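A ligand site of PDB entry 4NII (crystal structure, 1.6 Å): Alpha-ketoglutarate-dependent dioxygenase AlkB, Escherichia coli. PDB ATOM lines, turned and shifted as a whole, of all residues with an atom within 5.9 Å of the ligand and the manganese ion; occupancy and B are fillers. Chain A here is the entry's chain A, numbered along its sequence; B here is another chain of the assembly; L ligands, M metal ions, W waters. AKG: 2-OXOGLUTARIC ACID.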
ATOM      1  N   MET A  50      -9.884  -7.825 -27.007  1.00  0.00           N
ATOM      2  CA  MET A  50      -8.751  -6.939 -26.774  1.00  0.00           C
ATOM      3  C   MET A  50      -7.979  -6.614 -28.057  1.00  0.00           C
ATOM      4  O   MET A  50      -7.955  -7.409 -29.031  1.00  0.00           O
ATOM      5  CB  MET A  50      -7.782  -7.571 -25.785  1.00  0.00           C
ATOM      6  CG  MET A  50      -8.374  -7.631 -24.448  1.00  0.00           C
ATOM      7  SD  MET A  50      -7.348  -8.554 -23.276  1.00  0.00           S
ATOM      8  CE  MET A  50      -8.011  -8.072 -21.693  1.00  0.00           C
ATOM      9  N   LEU A 107      -3.685  -0.977 -23.783  1.00  0.00           N
ATOM     10  CA  LEU A 107      -4.541  -2.152 -24.006  1.00  0.00           C
ATOM     11  C   LEU A 107      -5.945  -1.672 -24.118  1.00  0.00           C
ATOM     12  O   LEU A 107      -6.434  -0.936 -23.261  1.00  0.00           O
ATOM     13  CB  LEU A 107      -4.422  -3.123 -22.858  1.00  0.00           C
ATOM     14  CG  LEU A 107      -5.339  -4.302 -22.748  1.00  0.00           C
ATOM     15  CD1 LEU A 107      -5.055  -5.291 -23.848  1.00  0.00           C
ATOM     16  CD2 LEU A 107      -5.187  -5.034 -21.426  1.00  0.00           C
ATOM     17  N   ASN A 109      -9.814  -2.681 -24.447  1.00  0.00           N
ATOM     18  CA  ASN A 109     -10.792  -3.710 -24.109  1.00  0.00           C
ATOM     19  C   ASN A 109     -12.191  -3.352 -24.632  1.00  0.00           C
ATOM     20  O   ASN A 109     -12.653  -2.237 -24.443  1.00  0.00           O
ATOM     21  CB  ASN A 109     -10.863  -3.849 -22.579  1.00  0.00           C
ATOM     22  CG  ASN A 109      -9.557  -4.297 -21.946  1.00  0.00           C
ATOM     23  OD1 ASN A 109      -9.092  -3.714 -20.968  1.00  0.00           O
ATOM     24  ND2 ASN A 109      -8.974  -5.327 -22.465  1.00  0.00           N
ATOM     25  N   TYR A 111     -16.066  -4.654 -24.132  1.00  0.00           N
ATOM     26  CA  TYR A 111     -17.014  -5.466 -23.380  1.00  0.00           C
ATOM     27  C   TYR A 111     -18.363  -5.459 -24.098  1.00  0.00           C
ATOM     28  O   TYR A 111     -18.985  -4.437 -24.223  1.00  0.00           O
ATOM     29  CB  TYR A 111     -17.254  -4.888 -22.003  1.00  0.00           C
ATOM     30  CG  TYR A 111     -16.016  -4.875 -21.128  1.00  0.00           C
ATOM     31  CD1 TYR A 111     -15.010  -3.926 -21.300  1.00  0.00           C
ATOM     32  CD2 TYR A 111     -15.861  -5.813 -20.128  1.00  0.00           C
ATOM     33  CE1 TYR A 111     -13.873  -3.946 -20.467  1.00  0.00           C
ATOM     34  CE2 TYR A 111     -14.763  -5.802 -19.272  1.00  0.00           C
ATOM     35  CZ  TYR A 111     -13.757  -4.896 -19.496  1.00  0.00           C
ATOM     36  OH  TYR A 111     -12.623  -4.903 -18.698  1.00  0.00           O
ATOM     37  N   LEU A 117     -14.147  -9.127 -16.427  1.00  0.00           N
ATOM     38  CA  LEU A 117     -12.751  -9.380 -16.197  1.00  0.00           C
ATOM     39  C   LEU A 117     -12.581  -9.694 -14.735  1.00  0.00           C
ATOM     40  O   LEU A 117     -12.734  -8.799 -13.896  1.00  0.00           O
ATOM     41  CB  LEU A 117     -11.950  -8.169 -16.623  1.00  0.00           C
ATOM     42  CG  LEU A 117     -10.481  -8.281 -16.897  1.00  0.00           C
ATOM     43  CD1 LEU A 117     -10.091  -9.430 -17.801  1.00  0.00           C
ATOM     44  CD2 LEU A 117      -9.915  -6.960 -17.441  1.00  0.00           C
ATOM     45  N   HIS A 120      -7.814  -9.422 -10.752  1.00  0.00           N
ATOM     46  CA  HIS A 120      -6.479  -9.697 -11.124  1.00  0.00           C
ATOM     47  C   HIS A 120      -5.636  -8.498 -10.743  1.00  0.00           C
ATOM     48  O   HIS A 120      -6.156  -7.463 -10.324  1.00  0.00           O
ATOM     49  CB  HIS A 120      -6.400  -9.941 -12.623  1.00  0.00           C
ATOM     50  CG  HIS A 120      -6.684  -8.723 -13.424  1.00  0.00           C
ATOM     51  ND1 HIS A 120      -7.961  -8.347 -13.784  1.00  0.00           N
ATOM     52  CD2 HIS A 120      -5.861  -7.762 -13.919  1.00  0.00           C
ATOM     53  CE1 HIS A 120      -7.910  -7.206 -14.437  1.00  0.00           C
ATOM     54  NE2 HIS A 120      -6.648  -6.866 -14.593  1.00  0.00           N
ATOM     55  N   GLN A 121      -4.319  -8.683 -10.799  1.00  0.00           N
ATOM     56  CA  GLN A 121      -3.340  -7.621 -10.590  1.00  0.00           C
ATOM     57  C   GLN A 121      -2.670  -7.318 -11.895  1.00  0.00           C
ATOM     58  O   GLN A 121      -2.463  -8.232 -12.721  1.00  0.00           O
ATOM     59  CB  GLN A 121      -2.282  -8.061  -9.607  1.00  0.00           C
ATOM     60  CG  GLN A 121      -2.803  -8.448  -8.252  1.00  0.00           C
ATOM     61  CD  GLN A 121      -1.678  -9.023  -7.376  1.00  0.00           C
ATOM     62  OE1 GLN A 121      -1.211 -10.139  -7.600  1.00  0.00           O
ATOM     63  NE2 GLN A 121      -1.191  -8.233  -6.466  1.00  0.00           N
ATOM     64  N   ASP A 122      -2.280  -6.063 -12.093  1.00  0.00           N
ATOM     65  CA  ASP A 122      -1.488  -5.696 -13.269  1.00  0.00           C
ATOM     66  C   ASP A 122      -0.016  -5.793 -12.862  1.00  0.00           C
ATOM     67  O   ASP A 122       0.529  -4.910 -12.175  1.00  0.00           O
ATOM     68  CB  ASP A 122      -1.808  -4.298 -13.804  1.00  0.00           C
ATOM     69  CG  ASP A 122      -3.028  -4.264 -14.671  1.00  0.00           C
ATOM     70  OD1 ASP A 122      -3.953  -5.057 -14.414  1.00  0.00           O
ATOM     71  OD2 ASP A 122      -3.066  -3.438 -15.635  1.00  0.00           O
ATOM     72  N   SER A 134      -6.665   4.295 -16.601  1.00  0.00           N
ATOM     73  CA  SER A 134      -7.727   3.428 -17.124  1.00  0.00           C
ATOM     74  C   SER A 134      -8.959   4.269 -17.462  1.00  0.00           C
ATOM     75  O   SER A 134      -9.575   4.845 -16.576  1.00  0.00           O
ATOM     76  CB  SER A 134      -8.064   2.382 -16.052  1.00  0.00           C
ATOM     77  OG  SER A 134      -8.921   1.389 -16.556  1.00  0.00           O
ATOM     78  N   SER A 136     -12.738   4.780 -19.254  1.00  0.00           N
ATOM     79  CA  SER A 136     -13.997   4.069 -19.555  1.00  0.00           C
ATOM     80  C   SER A 136     -14.731   4.827 -20.662  1.00  0.00           C
ATOM     81  O   SER A 136     -14.855   6.081 -20.591  1.00  0.00           O
ATOM     82  CB  SER A 136     -14.936   4.033 -18.354  1.00  0.00           C
ATOM     83  OG  SER A 136     -14.341   3.274 -17.309  1.00  0.00           O
ATOM     84  N   PHE A 143     -16.840  -1.672 -11.422  1.00  0.00           N
ATOM     85  CA  PHE A 143     -15.422  -1.876 -11.289  1.00  0.00           C
ATOM     86  C   PHE A 143     -15.224  -2.284  -9.860  1.00  0.00           C
ATOM     87  O   PHE A 143     -15.790  -1.642  -9.013  1.00  0.00           O
ATOM     88  CB  PHE A 143     -14.713  -0.564 -11.560  1.00  0.00           C
ATOM     89  CG  PHE A 143     -13.232  -0.597 -11.419  1.00  0.00           C
ATOM     90  CD1 PHE A 143     -12.434  -1.391 -12.241  1.00  0.00           C
ATOM     91  CD2 PHE A 143     -12.592   0.283 -10.556  1.00  0.00           C
ATOM     92  CE1 PHE A 143     -11.059  -1.364 -12.131  1.00  0.00           C
ATOM     93  CE2 PHE A 143     -11.192   0.342 -10.466  1.00  0.00           C
ATOM     94  CZ  PHE A 143     -10.440  -0.509 -11.234  1.00  0.00           C
ATOM     95  N   LEU A 159     -18.448   2.745 -13.116  1.00  0.00           N
ATOM     96  CA  LEU A 159     -17.660   3.571 -14.021  1.00  0.00           C
ATOM     97  C   LEU A 159     -18.533   3.908 -15.231  1.00  0.00           C
ATOM     98  O   LEU A 159     -19.084   3.030 -15.925  1.00  0.00           O
ATOM     99  CB  LEU A 159     -16.398   2.860 -14.462  1.00  0.00           C
ATOM    100  CG  LEU A 159     -15.428   2.486 -13.347  1.00  0.00           C
ATOM    101  CD1 LEU A 159     -14.166   1.825 -13.893  1.00  0.00           C
ATOM    102  CD2 LEU A 159     -15.066   3.752 -12.603  1.00  0.00           C
ATOM    103  N   TRP A 167      -4.331   4.424 -10.771  1.00  0.00           N
ATOM    104  CA  TRP A 167      -3.733   3.852  -9.583  1.00  0.00           C
ATOM    105  C   TRP A 167      -2.238   3.674  -9.725  1.00  0.00           C
ATOM    106  O   TRP A 167      -1.695   3.524 -10.823  1.00  0.00           O
ATOM    107  CB  TRP A 167      -4.472   2.615  -9.067  1.00  0.00           C
ATOM    108  CG  TRP A 167      -4.491   1.392  -9.898  1.00  0.00           C
ATOM    109  CD1 TRP A 167      -3.778   0.249  -9.702  1.00  0.00           C
ATOM    110  CD2 TRP A 167      -5.382   1.127 -10.968  1.00  0.00           C
ATOM    111  NE1 TRP A 167      -4.141  -0.713 -10.601  1.00  0.00           N
ATOM    112  CE2 TRP A 167      -5.120  -0.186 -11.418  1.00  0.00           C
ATOM    113  CE3 TRP A 167      -6.383   1.864 -11.591  1.00  0.00           C
ATOM    114  CZ2 TRP A 167      -5.819  -0.763 -12.471  1.00  0.00           C
ATOM    115  CZ3 TRP A 167      -7.061   1.310 -12.635  1.00  0.00           C
ATOM    116  CH2 TRP A 167      -6.777   0.007 -13.071  1.00  0.00           C
ATOM    117  N   HIS A 176      -8.176  -5.850  -8.922  1.00  0.00           N
ATOM    118  CA  HIS A 176      -9.293  -5.108  -9.493  1.00  0.00           C
ATOM    119  C   HIS A 176      -9.911  -5.943 -10.616  1.00  0.00           C
ATOM    120  O   HIS A 176      -9.336  -6.949 -11.084  1.00  0.00           O
ATOM    121  CB  HIS A 176      -8.817  -3.761 -10.014  1.00  0.00           C
ATOM    122  CG  HIS A 176      -7.759  -3.889 -11.047  1.00  0.00           C
ATOM    123  ND1 HIS A 176      -6.450  -4.189 -10.733  1.00  0.00           N
ATOM    124  CD2 HIS A 176      -7.824  -3.877 -12.391  1.00  0.00           C
ATOM    125  CE1 HIS A 176      -5.743  -4.303 -11.846  1.00  0.00           C
ATOM    126  NE2 HIS A 176      -6.553  -4.100 -12.865  1.00  0.00           N
ATOM    127  N   GLY A 177     -11.085  -5.506 -11.067  1.00  0.00           N
ATOM    128  CA  GLY A 177     -11.823  -6.293 -12.037  1.00  0.00           C
ATOM    129  C   GLY A 177     -13.087  -5.581 -12.444  1.00  0.00           C
ATOM    130  O   GLY A 177     -13.392  -4.499 -11.906  1.00  0.00           O
ATOM    131  N   ILE A 178     -13.785  -6.209 -13.379  1.00  0.00           N
ATOM    132  CA  ILE A 178     -15.048  -5.718 -13.939  1.00  0.00           C
ATOM    133  C   ILE A 178     -16.122  -6.797 -13.893  1.00  0.00           C
ATOM    134  O   ILE A 178     -15.908  -7.948 -14.313  1.00  0.00           O
ATOM    135  CB  ILE A 178     -14.865  -5.234 -15.384  1.00  0.00           C
ATOM    136  CG1 ILE A 178     -13.941  -4.013 -15.492  1.00  0.00           C
ATOM    137  CG2 ILE A 178     -16.215  -4.954 -16.038  1.00  0.00           C
ATOM    138  CD1 ILE A 178     -14.529  -2.737 -15.025  1.00  0.00           C
ATOM    139  N   ARG A 193     -19.035  -1.423 -24.060  1.00  0.00           N
ATOM    140  CA  ARG A 193     -18.131  -0.583 -23.288  1.00  0.00           C
ATOM    141  C   ARG A 193     -16.703  -0.811 -23.793  1.00  0.00           C
ATOM    142  O   ARG A 193     -16.323  -1.930 -24.158  1.00  0.00           O
ATOM    143  CB  ARG A 193     -18.199  -0.949 -21.811  1.00  0.00           C
ATOM    144  CG  ARG A 193     -17.127  -0.296 -20.944  1.00  0.00           C
ATOM    145  CD  ARG A 193     -17.318  -0.606 -19.470  1.00  0.00           C
ATOM    146  NE  ARG A 193     -16.356   0.144 -18.653  1.00  0.00           N
ATOM    147  CZ  ARG A 193     -15.189  -0.333 -18.233  1.00  0.00           C
ATOM    148  NH1 ARG A 193     -14.802  -1.561 -18.546  1.00  0.00           N
ATOM    149  NH2 ARG A 193     -14.394   0.443 -17.497  1.00  0.00           N
ATOM    150  N   ASN A 195     -12.635   0.090 -22.679  1.00  0.00           N
ATOM    151  CA  ASN A 195     -11.686   0.648 -21.737  1.00  0.00           C
ATOM    152  C   ASN A 195     -10.311   0.775 -22.394  1.00  0.00           C
ATOM    153  O   ASN A 195      -9.894  -0.087 -23.136  1.00  0.00           O
ATOM    154  CB  ASN A 195     -11.667  -0.248 -20.500  1.00  0.00           C
ATOM    155  CG  ASN A 195     -10.841   0.336 -19.385  1.00  0.00           C
ATOM    156  OD1 ASN A 195      -9.711  -0.030 -19.221  1.00  0.00           O
ATOM    157  ND2 ASN A 195     -11.410   1.212 -18.612  1.00  0.00           N
ATOM    158  N   THR A 197      -6.366   1.019 -21.177  1.00  0.00           N
ATOM    159  CA  THR A 197      -5.438   0.816 -20.045  1.00  0.00           C
ATOM    160  C   THR A 197      -4.040   1.206 -20.491  1.00  0.00           C
ATOM    161  O   THR A 197      -3.459   0.533 -21.340  1.00  0.00           O
ATOM    162  CB  THR A 197      -5.480  -0.629 -19.627  1.00  0.00           C
ATOM    163  OG1 THR A 197      -6.782  -0.895 -19.084  1.00  0.00           O
ATOM    164  CG2 THR A 197      -4.464  -0.847 -18.512  1.00  0.00           C
ATOM    165  P   6MA B   8      -5.545 -14.031 -13.211  1.00  0.00           P
ATOM    166  OP1 6MA B   8      -4.298 -14.067 -14.016  1.00  0.00           O
ATOM    167  OP2 6MA B   8      -5.773 -13.072 -12.106  1.00  0.00           O
ATOM    168  O5' 6MA B   8      -6.675 -13.680 -14.382  1.00  0.00           O
ATOM    169  C5' 6MA B   8      -7.960 -13.240 -13.996  1.00  0.00           C
ATOM    170  C4' 6MA B   8      -8.558 -12.563 -15.215  1.00  0.00           C
ATOM    171  O4' 6MA B   8      -7.801 -11.361 -15.414  1.00  0.00           O
ATOM    172  C3' 6MA B   8      -8.432 -13.404 -16.440  1.00  0.00           C
ATOM    173  O3' 6MA B   8      -9.471 -13.077 -17.415  1.00  0.00           O
ATOM    174  C2' 6MA B   8      -7.134 -12.907 -17.028  1.00  0.00           C
ATOM    175  C1' 6MA B   8      -7.161 -11.409 -16.692  1.00  0.00           C
ATOM    176  N9  6MA B   8      -5.851 -10.764 -16.580  1.00  0.00           N
ATOM    177  C8  6MA B   8      -4.874 -11.166 -15.721  1.00  0.00           C
ATOM    178  N7  6MA B   8      -3.843 -10.326 -15.800  1.00  0.00           N
ATOM    179  C5  6MA B   8      -4.174  -9.309 -16.638  1.00  0.00           C
ATOM    180  C6  6MA B   8      -3.516  -8.076 -17.096  1.00  0.00           C
ATOM    181  N1  6MA B   8      -4.191  -7.258 -17.946  1.00  0.00           N
ATOM    182  C2  6MA B   8      -5.431  -7.576 -18.326  1.00  0.00           C
ATOM    183  N3  6MA B   8      -6.090  -8.702 -17.955  1.00  0.00           N
ATOM    184  C4  6MA B   8      -5.513  -9.581 -17.107  1.00  0.00           C
ATOM    185  N6  6MA B   8      -2.257  -7.875 -16.636  1.00  0.00           N
ATOM    186  C1  6MA B   8      -1.423  -6.759 -17.145  1.00  0.00           C
HETATM  187  C1  AKG L   1      -7.251  -4.394 -17.713  1.00  0.00           C
HETATM  188  O1  AKG L   1      -6.155  -4.792 -17.167  1.00  0.00           O
HETATM  189  O2  AKG L   1      -7.482  -4.399 -18.956  1.00  0.00           O
HETATM  190  C2  AKG L   1      -8.328  -3.906 -16.846  1.00  0.00           C
HETATM  191  O5  AKG L   1      -8.214  -4.053 -15.651  1.00  0.00           O
HETATM  192  C3  AKG L   1      -9.578  -3.273 -17.442  1.00  0.00           C
HETATM  193  C4  AKG L   1     -10.418  -2.557 -16.390  1.00  0.00           C
HETATM  194  C5  AKG L   1     -11.612  -1.862 -17.019  1.00  0.00           C
HETATM  195  O3  AKG L   1     -12.050  -0.833 -16.474  1.00  0.00           O
HETATM  196  O4  AKG L   1     -12.152  -2.345 -18.033  1.00  0.00           O
HETATM  197 MN    MN M   1      -6.032  -4.746 -14.965  1.00  0.00          MN
HETATM  198  O   HOH W   1      -7.253  -1.055 -16.402  1.00  0.00           O
HETATM  199  O   HOH W   2      -3.833  -4.592 -18.117  1.00  0.00           O
HETATM  200  O   HOH W   3      -5.488  -2.450 -15.291  1.00  0.00           O
HETATM  201  O   HOH W   4     -10.983   0.955 -14.786  1.00  0.00           O
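The manganese ion is bound by OD1 of Asp 122 (2.2 Å).
O1 of the ligand binds the manganese ion (2.2 Å).
A ring nitrogen (NE2) of His 120 binds the manganese ion (2.2 Å).
NE2 of His 176 binds the manganese ion (2.3 Å).
Water W3 binds the manganese ion (2.4 Å).
The manganese ion is bound by an oxygen (O5) of the ligand, at 2.4 Å.
Water W2 bridges N1 of 6MA 8 of chain B and OD2 of Asp 122.
Water W4 bridges an oxygen (O3) of the ligand (2.7 Å) and the side-chain hydroxyl (OG) of Ser 134 (2.8 Å).
Water W1 lies within hydrogen-bond range of the side-chain hydroxyl of Thr 197 (2.7 Å) and the side-chain hydroxyl of Ser 134 (3.0 Å).
Within 4 Å of the manganese ion: His 120, Asp 122 and His 176.
The nearest printed residue that does not touch the manganese ion is 6MA 8 of chain B (4.3 Å).
O4' of 6MA 8 of chain B is in hydrogen-bond range of a ring nitrogen (ND1) of His 120.
The side-chain sulfur (SD) of Met 50 sits close to the side-chain amide nitrogen (ND2) of Asn 109 (3.7 Å).
N of Tyr 111 lies within hydrogen-bond range of O of Arg 193 (2.7 Å).
The guanidinium group (NH2) of Arg 193 sits close to the side-chain amide nitrogen (ND2) of Asn 195 (3.3 Å).
The guanidinium group of Arg 193 is in hydrogen-bond range of the side-chain hydroxyl of Ser 136 (2.8 Å).
OD1 of Asn 195 is in hydrogen-bond range of OG1 of Thr 197 (3.1 Å).
The backbone carbonyl oxygen (O) of Leu 107 sits at hydrogen-bond distance from the backbone NH (N) of Thr 197.
O of Leu 117 is in hydrogen-bond range of N of Ile 178, 2.8 Å away.
N1 of 6MA 8 of chain B sits close to an oxygen (O1) of the ligand (3.2 Å).
Residues that only touch the ligand: Leu 107 (3.4 Å), Leu 117 (3.5 Å), Ser 134 (3.8 Å), Ile 178 (3.4 Å) and Thr 197 (3.6 Å).
Hydrophobic or aromatic side chains within 4 Å of the ligand: Leu 107, Tyr 111, Leu 117, His 120, His 176 and Ile 178.
Within 4 Å of the ligand: Leu 107, Asn 109, Tyr 111, Leu 117, His 120, Asp 122, Ser 134, His 176, Ile 178, Arg 193, Asn 195, Thr 197 and 6MA 8 of chain B.
The nearest printed residue that does not touch the ligand is Leu 159 (4.3 Å).
The side-chain amide oxygen (OD1) of Asn 109 lies close to an oxygen (O2) of the ligand (2.7 Å).
An oxygen (O4) of the ligand lies within hydrogen-bond range of the side-chain hydroxyl of Tyr 111 (2.7 Å).
The guanidinium group (NH1) of Arg 193 lies within salt-bridge range of an oxygen (O4) of the ligand, at 2.8 Å.
ND2 of Asn 195 lies within hydrogen-bond range of O3 of the ligand.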
